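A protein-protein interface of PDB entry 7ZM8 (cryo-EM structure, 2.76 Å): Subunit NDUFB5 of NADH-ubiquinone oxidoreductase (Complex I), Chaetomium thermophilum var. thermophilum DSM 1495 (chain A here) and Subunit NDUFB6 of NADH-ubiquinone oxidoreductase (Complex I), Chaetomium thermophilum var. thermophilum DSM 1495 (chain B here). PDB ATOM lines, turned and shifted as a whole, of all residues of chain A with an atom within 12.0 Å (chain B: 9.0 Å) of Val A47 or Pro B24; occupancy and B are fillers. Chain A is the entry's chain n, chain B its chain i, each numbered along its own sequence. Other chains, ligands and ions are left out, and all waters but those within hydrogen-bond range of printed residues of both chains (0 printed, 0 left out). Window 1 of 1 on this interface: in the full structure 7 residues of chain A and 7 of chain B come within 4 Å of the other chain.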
ATOM      1  N   GLY A  44       7.016 -21.814  -2.312  1.00  0.00           N
ATOM      2  CA  GLY A  44       8.211 -20.981  -2.547  1.00  0.00           C
ATOM      3  C   GLY A  44       8.587 -20.936  -4.017  1.00  0.00           C
ATOM      4  O   GLY A  44       8.134 -21.824  -4.765  1.00  0.00           O
ATOM      5  N   HIS A  45       9.380 -19.936  -4.408  1.00  0.00           N
ATOM      6  CA  HIS A  45       9.754 -19.771  -5.835  1.00  0.00           C
ATOM      7  C   HIS A  45      10.883 -20.734  -6.193  1.00  0.00           C
ATOM      8  O   HIS A  45      11.433 -21.367  -5.274  1.00  0.00           O
ATOM      9  CB  HIS A  45      10.145 -18.318  -6.121  1.00  0.00           C
ATOM     10  CG  HIS A  45      11.397 -17.897  -5.432  1.00  0.00           C
ATOM     11  ND1 HIS A  45      12.639 -18.036  -6.012  1.00  0.00           N
ATOM     12  CD2 HIS A  45      11.604 -17.351  -4.216  1.00  0.00           C
ATOM     13  CE1 HIS A  45      13.559 -17.597  -5.183  1.00  0.00           C
ATOM     14  NE2 HIS A  45      12.949 -17.171  -4.075  1.00  0.00           N
ATOM     15  N   ASN A  46      11.215 -20.824  -7.478  1.00  0.00           N
ATOM     16  CA  ASN A  46      12.292 -21.701  -7.947  1.00  0.00           C
ATOM     17  C   ASN A  46      13.317 -20.850  -8.678  1.00  0.00           C
ATOM     18  O   ASN A  46      14.259 -21.423  -9.189  1.00  0.00           O
ATOM     19  CB  ASN A  46      11.712 -22.798  -8.831  1.00  0.00           C
ATOM     20  CG  ASN A  46      10.603 -23.569  -8.147  1.00  0.00           C
ATOM     21  OD1 ASN A  46      10.791 -24.102  -7.056  1.00  0.00           O
ATOM     22  ND2 ASN A  46       9.444 -23.633  -8.781  1.00  0.00           N
ATOM     23  N   VAL A  47      13.091 -19.550  -8.787  1.00  0.00           N
ATOM     24  CA  VAL A  47      14.025 -18.716  -9.585  1.00  0.00           C
ATOM     25  C   VAL A  47      15.400 -18.915  -8.981  1.00  0.00           C
ATOM     26  O   VAL A  47      15.541 -18.797  -7.761  1.00  0.00           O
ATOM     27  CB  VAL A  47      13.653 -17.226  -9.569  1.00  0.00           C
ATOM     28  CG1 VAL A  47      14.601 -16.394 -10.417  1.00  0.00           C
ATOM     29  CG2 VAL A  47      12.214 -17.004 -10.003  1.00  0.00           C
ATOM     30  N   GLU A  48      16.370 -19.253  -9.827  1.00  0.00           N
ATOM     31  CA  GLU A  48      17.738 -19.523  -9.340  1.00  0.00           C
ATOM     32  C   GLU A  48      18.664 -18.465  -9.930  1.00  0.00           C
ATOM     33  O   GLU A  48      18.444 -18.067 -11.083  1.00  0.00           O
ATOM     34  CB  GLU A  48      18.129 -20.945  -9.727  1.00  0.00           C
ATOM     35  CG  GLU A  48      17.467 -22.003  -8.866  1.00  0.00           C
ATOM     36  CD  GLU A  48      18.058 -23.396  -8.996  1.00  0.00           C
ATOM     37  OE1 GLU A  48      18.914 -23.594  -9.882  1.00  0.00           O
ATOM     38  OE2 GLU A  48      17.667 -24.277  -8.205  1.00  0.00           O
ATOM     39  N   GLU A  49      19.650 -18.023  -9.153  1.00  0.00           N
ATOM     40  CA  GLU A  49      20.614 -17.005  -9.625  1.00  0.00           C
ATOM     41  C   GLU A  49      21.926 -17.713  -9.936  1.00  0.00           C
ATOM     42  O   GLU A  49      22.436 -18.406  -9.045  1.00  0.00           O
ATOM     43  CB  GLU A  49      20.864 -15.989  -8.506  1.00  0.00           C
ATOM     44  CG  GLU A  49      21.890 -14.922  -8.837  1.00  0.00           C
ATOM     45  CD  GLU A  49      21.384 -13.808  -9.735  1.00  0.00           C
ATOM     46  OE1 GLU A  49      20.154 -13.677  -9.877  1.00  0.00           O
ATOM     47  OE2 GLU A  49      22.222 -13.075 -10.290  1.00  0.00           O
ATOM     48  N   PRO A  50      22.504 -17.582 -11.148  1.00  0.00           N
ATOM     49  CA  PRO A  50      23.820 -18.161 -11.411  1.00  0.00           C
ATOM     50  C   PRO A  50      24.931 -17.420 -10.653  1.00  0.00           C
ATOM     51  O   PRO A  50      24.718 -16.296 -10.283  1.00  0.00           O
ATOM     52  CB  PRO A  50      23.968 -18.003 -12.928  1.00  0.00           C
ATOM     53  CG  PRO A  50      23.078 -16.829 -13.275  1.00  0.00           C
ATOM     54  CD  PRO A  50      21.918 -16.913 -12.306  1.00  0.00           C
ATOM     55  N   LEU A  51      26.083 -18.065 -10.459  1.00  0.00           N
ATOM     56  CA  LEU A  51      27.224 -17.457  -9.712  1.00  0.00           C
ATOM     57  C   LEU A  51      27.699 -16.188 -10.402  1.00  0.00           C
ATOM     58  O   LEU A  51      28.195 -15.312  -9.707  1.00  0.00           O
ATOM     59  CB  LEU A  51      28.361 -18.445  -9.441  1.00  0.00           C
ATOM     60  CG  LEU A  51      28.249 -19.221  -8.137  1.00  0.00           C
ATOM     61  CD1 LEU A  51      29.243 -20.364  -8.109  1.00  0.00           C
ATOM     62  CD2 LEU A  51      28.446 -18.300  -6.947  1.00  0.00           C
ATOM     63  N   GLY A  52      27.620 -16.117 -11.720  1.00  0.00           N
ATOM     64  CA  GLY A  52      27.934 -14.844 -12.396  1.00  0.00           C
ATOM     65  C   GLY A  52      29.323 -14.768 -12.982  1.00  0.00           C
ATOM     66  O   GLY A  52      30.192 -15.533 -12.577  1.00  0.00           O
ATOM     67  N   ALA B  17      23.652  -6.587  -4.021  1.00  0.00           N
ATOM     68  CA  ALA B  17      23.355  -7.106  -2.696  1.00  0.00           C
ATOM     69  C   ALA B  17      22.000  -7.787  -2.626  1.00  0.00           C
ATOM     70  O   ALA B  17      21.591  -8.215  -1.549  1.00  0.00           O
ATOM     71  CB  ALA B  17      23.431  -5.985  -1.664  1.00  0.00           C
ATOM     72  N   GLY B  18      21.298  -7.896  -3.755  1.00  0.00           N
ATOM     73  CA  GLY B  18      20.055  -8.622  -3.856  1.00  0.00           C
ATOM     74  C   GLY B  18      18.841  -7.737  -4.045  1.00  0.00           C
ATOM     75  O   GLY B  18      17.985  -8.050  -4.877  1.00  0.00           O
ATOM     76  N   TYR B  21      14.016  -8.461  -1.116  1.00  0.00           N
ATOM     77  CA  TYR B  21      13.843  -9.671  -0.263  1.00  0.00           C
ATOM     78  C   TYR B  21      14.478 -10.798  -1.046  1.00  0.00           C
ATOM     79  O   TYR B  21      13.852 -11.850  -1.169  1.00  0.00           O
ATOM     80  CB  TYR B  21      12.373  -9.935   0.065  1.00  0.00           C
ATOM     81  CG  TYR B  21      11.713  -8.883   0.919  1.00  0.00           C
ATOM     82  CD1 TYR B  21      11.866  -8.885   2.294  1.00  0.00           C
ATOM     83  CD2 TYR B  21      10.951  -7.875   0.351  1.00  0.00           C
ATOM     84  CE1 TYR B  21      11.273  -7.919   3.087  1.00  0.00           C
ATOM     85  CE2 TYR B  21      10.356  -6.896   1.128  1.00  0.00           C
ATOM     86  CZ  TYR B  21      10.515  -6.923   2.501  1.00  0.00           C
ATOM     87  OH  TYR B  21       9.926  -5.977   3.284  1.00  0.00           O
ATOM     88  N   ALA B  22      15.714 -10.613  -1.485  1.00  0.00           N
ATOM     89  CA  ALA B  22      16.236 -11.586  -2.456  1.00  0.00           C
ATOM     90  C   ALA B  22      16.906 -12.812  -1.857  1.00  0.00           C
ATOM     91  O   ALA B  22      17.956 -12.667  -1.212  1.00  0.00           O
ATOM     92  CB  ALA B  22      17.124 -10.880  -3.441  1.00  0.00           C
ATOM     93  N   GLN B  23      16.287 -13.968  -2.064  1.00  0.00           N
ATOM     94  CA  GLN B  23      16.938 -15.237  -1.690  1.00  0.00           C
ATOM     95  C   GLN B  23      16.751 -16.121  -2.915  1.00  0.00           C
ATOM     96  O   GLN B  23      15.598 -16.342  -3.288  1.00  0.00           O
ATOM     97  CB  GLN B  23      16.292 -15.840  -0.451  1.00  0.00           C
ATOM     98  CG  GLN B  23      16.751 -17.252  -0.142  1.00  0.00           C
ATOM     99  CD  GLN B  23      16.906 -17.407   1.347  1.00  0.00           C
ATOM    100  OE1 GLN B  23      17.437 -16.528   2.018  1.00  0.00           O
ATOM    101  NE2 GLN B  23      16.428 -18.521   1.875  1.00  0.00           N
ATOM    102  N   PRO B  24      17.816 -16.600  -3.580  1.00  0.00           N
ATOM    103  CA  PRO B  24      17.641 -17.516  -4.696  1.00  0.00           C
ATOM    104  C   PRO B  24      17.244 -18.913  -4.204  1.00  0.00           C
ATOM    105  O   PRO B  24      17.376 -19.171  -3.030  1.00  0.00           O
ATOM    106  CB  PRO B  24      19.002 -17.466  -5.398  1.00  0.00           C
ATOM    107  CG  PRO B  24      19.981 -17.086  -4.315  1.00  0.00           C
ATOM    108  CD  PRO B  24      19.206 -16.222  -3.347  1.00  0.00           C
ATOM    109  N   ALA B  25      16.737 -19.763  -5.098  1.00  0.00           N
ATOM    110  CA  ALA B  25      16.428 -21.148  -4.684  1.00  0.00           C
ATOM    111  C   ALA B  25      17.722 -21.959  -4.718  1.00  0.00           C
ATOM    112  O   ALA B  25      17.755 -23.018  -4.073  1.00  0.00           O
ATOM    113  CB  ALA B  25      15.392 -21.725  -5.602  1.00  0.00           C
ATOM    114  N   ASN B  26      18.752 -21.471  -5.407  1.00  0.00           N
ATOM    115  CA  ASN B  26      20.076 -22.140  -5.389  1.00  0.00           C
ATOM    116  C   ASN B  26      20.929 -21.554  -4.277  1.00  0.00           C
ATOM    117  O   ASN B  26      22.114 -21.873  -4.247  1.00  0.00           O
ATOM    118  CB  ASN B  26      20.811 -22.067  -6.718  1.00  0.00           C
ATOM    119  CG  ASN B  26      20.714 -20.759  -7.451  1.00  0.00           C
ATOM    120  OD1 ASN B  26      20.203 -19.775  -6.933  1.00  0.00           O
ATOM    121  ND2 ASN B  26      21.204 -20.758  -8.675  1.00  0.00           N
ATOM    122  N   TRP B  27      20.326 -20.791  -3.360  1.00  0.00           N
ATOM    123  CA  TRP B  27      21.107 -20.066  -2.326  1.00  0.00           C
ATOM    124  C   TRP B  27      22.097 -20.999  -1.630  1.00  0.00           C
ATOM    125  O   TRP B  27      23.240 -20.572  -1.427  1.00  0.00           O
ATOM    126  CB  TRP B  27      20.190 -19.311  -1.356  1.00  0.00           C
ATOM    127  CG  TRP B  27      19.576 -20.086  -0.231  1.00  0.00           C
ATOM    128  CD1 TRP B  27      18.307 -20.581  -0.169  1.00  0.00           C
ATOM    129  CD2 TRP B  27      20.186 -20.396   1.034  1.00  0.00           C
ATOM    130  NE1 TRP B  27      18.094 -21.199   1.033  1.00  0.00           N
ATOM    131  CE2 TRP B  27      19.229 -21.102   1.791  1.00  0.00           C
ATOM    132  CE3 TRP B  27      21.446 -20.164   1.592  1.00  0.00           C
ATOM    133  CZ2 TRP B  27      19.499 -21.572   3.074  1.00  0.00           C
ATOM    134  CZ3 TRP B  27      21.715 -20.639   2.855  1.00  0.00           C
ATOM    135  CH2 TRP B  27      20.752 -21.332   3.585  1.00  0.00           C
ATOM    136  N   LYS B  28      21.674 -22.217  -1.290  1.00  0.00           N
ATOM    137  CA  LYS B  28      22.543 -23.121  -0.546  1.00  0.00           C
ATOM    138  C   LYS B  28      23.745 -23.535  -1.378  1.00  0.00           C
ATOM    139  O   LYS B  28      24.855 -23.665  -0.853  1.00  0.00           O
ATOM    140  CB  LYS B  28      21.762 -24.349  -0.097  1.00  0.00           C
ATOM    141  CG  LYS B  28      20.688 -24.064   0.918  1.00  0.00           C
ATOM    142  CD  LYS B  28      20.034 -25.339   1.390  1.00  0.00           C
ATOM    143  CE  LYS B  28      19.019 -25.074   2.486  1.00  0.00           C
ATOM    144  NZ  LYS B  28      17.737 -24.539   1.949  1.00  0.00           N
ATOM    145  N   GLN B  29      23.548 -23.793  -2.658  1.00  0.00           N
ATOM    146  CA  GLN B  29      24.664 -24.247  -3.517  1.00  0.00           C
ATOM    147  C   GLN B  29      25.667 -23.121  -3.660  1.00  0.00           C
ATOM    148  O   GLN B  29      26.843 -23.348  -3.441  1.00  0.00           O
ATOM    149  CB  GLN B  29      24.143 -24.623  -4.890  1.00  0.00           C
ATOM    150  CG  GLN B  29      23.446 -25.975  -4.932  1.00  0.00           C
ATOM    151  CD  GLN B  29      22.052 -25.956  -4.355  1.00  0.00           C
ATOM    152  OE1 GLN B  29      21.801 -26.468  -3.268  1.00  0.00           O
ATOM    153  NE2 GLN B  29      21.126 -25.362  -5.088  1.00  0.00           N
ATOM    154  N   ASN B  30      25.198 -21.943  -4.007  1.00  0.00           N
ATOM    155  CA  ASN B  30      26.068 -20.768  -4.158  1.00  0.00           C
ATOM    156  C   ASN B  30      26.791 -20.489  -2.833  1.00  0.00           C
ATOM    157  O   ASN B  30      27.988 -20.240  -2.885  1.00  0.00           O
ATOM    158  CB  ASN B  30      25.214 -19.608  -4.664  1.00  0.00           C
ATOM    159  CG  ASN B  30      24.850 -19.683  -6.128  1.00  0.00           C
ATOM    160  OD1 ASN B  30      24.086 -18.865  -6.623  1.00  0.00           O
ATOM    161  ND2 ASN B  30      25.390 -20.660  -6.831  1.00  0.00           N
ATOM    162  N   THR B  31      26.113 -20.556  -1.690  1.00  0.00           N
ATOM    163  CA  THR B  31      26.693 -20.299  -0.345  1.00  0.00           C
ATOM    164  C   THR B  31      27.741 -21.348  -0.042  1.00  0.00           C
ATOM    165  O   THR B  31      28.781 -20.979   0.524  1.00  0.00           O
ATOM    166  CB  THR B  31      25.629 -20.295   0.748  1.00  0.00           C
ATOM    167  OG1 THR B  31      24.755 -19.218   0.420  1.00  0.00           O
ATOM    168  CG2 THR B  31      26.182 -20.100   2.140  1.00  0.00           C
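NE1 of Trp B27 lies close to NE2 of Gln B23 (3.3 Å).
A ring nitrogen (ND1) of His A45 sits at hydrogen-bond distance from the backbone NH (N) of Val A47, at 3.2 Å.
Hydrophobic or aromatic side chains of chain A within 4 Å of the printed part of chain B: His A45 and Leu A51.
Of the 13 printed residues of chain B, 5 touch a printed residue of chain A.
Printed residues of chain B that touch a printed residue of chain A: Gln B23, Pro B24, Ala B25, Asn B26 and Asn B30.
Hydrophobic or aromatic side chains of chain B that line the printed part of chain A: Pro B24 and Ala B25.
Among the printed residues, 11 pairs touch across the chains.
Among the printed residues, no Asp or Glu carboxylate lies within 4 Å of a Lys or Arg side-chain nitrogen of the other chain.
His A45 touches Ala B25 (CE1 to N, 3.8 Å).
Ala B25 touches Asn A46 (CB to O, 3.8 Å).
Val A47 touches Pro B24 (O to CA, 3.9 Å).
CG of Glu A48 touches CB of Ala B25, at 3.9 Å.
CB of Glu A48 touches ND2 of Asn B26, at 3.3 Å.
Glu A49 touches Pro B24.
Leu A51 touches Asn B30.
Of the printed residues of chain B, Asn A46 touches Ala B25 (3.8 Å).
Val A47 touches just these residues of chain B: Pro B24 and Ala B25.
Printed residues of chain B within 4 Å of Leu A51: Asn B30.
No residue of chain A comes within 4 Å of Ala B22.
Of chain A, only His A45 (2.9 Å) comes within 4 Å of Gln B23.
Ala B25 touches four residues of chain A.
Of chain A, only Glu A48 and Glu A49 come within 4 Å of Asn B26.
No residue of chain A comes within 4 Å of Trp B27.
Gln B29 touches none of the printed residues of chain A.
Of the printed residues of chain A, Asn B30 touches Glu A49 (3.0 Å) and Leu A51 (3.5 Å).
A ring nitrogen (NE2) of His A45 lies within hydrogen-bond range of the backbone carbonyl oxygen of Gln B23, 2.9 Å away.
The backbone carbonyl oxygen (O) of Val A47 sits at hydrogen-bond distance from the backbone NH (N) of Ala B25 (3.1 Å).
The side-chain amide nitrogen (ND2) of Asn B26 is in hydrogen-bond range of the backbone carbonyl oxygen (O) of Glu A49, at 2.7 Å.
The side-chain amide oxygen (OD1) of Asn B30 sits close to the backbone carbonyl oxygen (O) of Glu A49.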
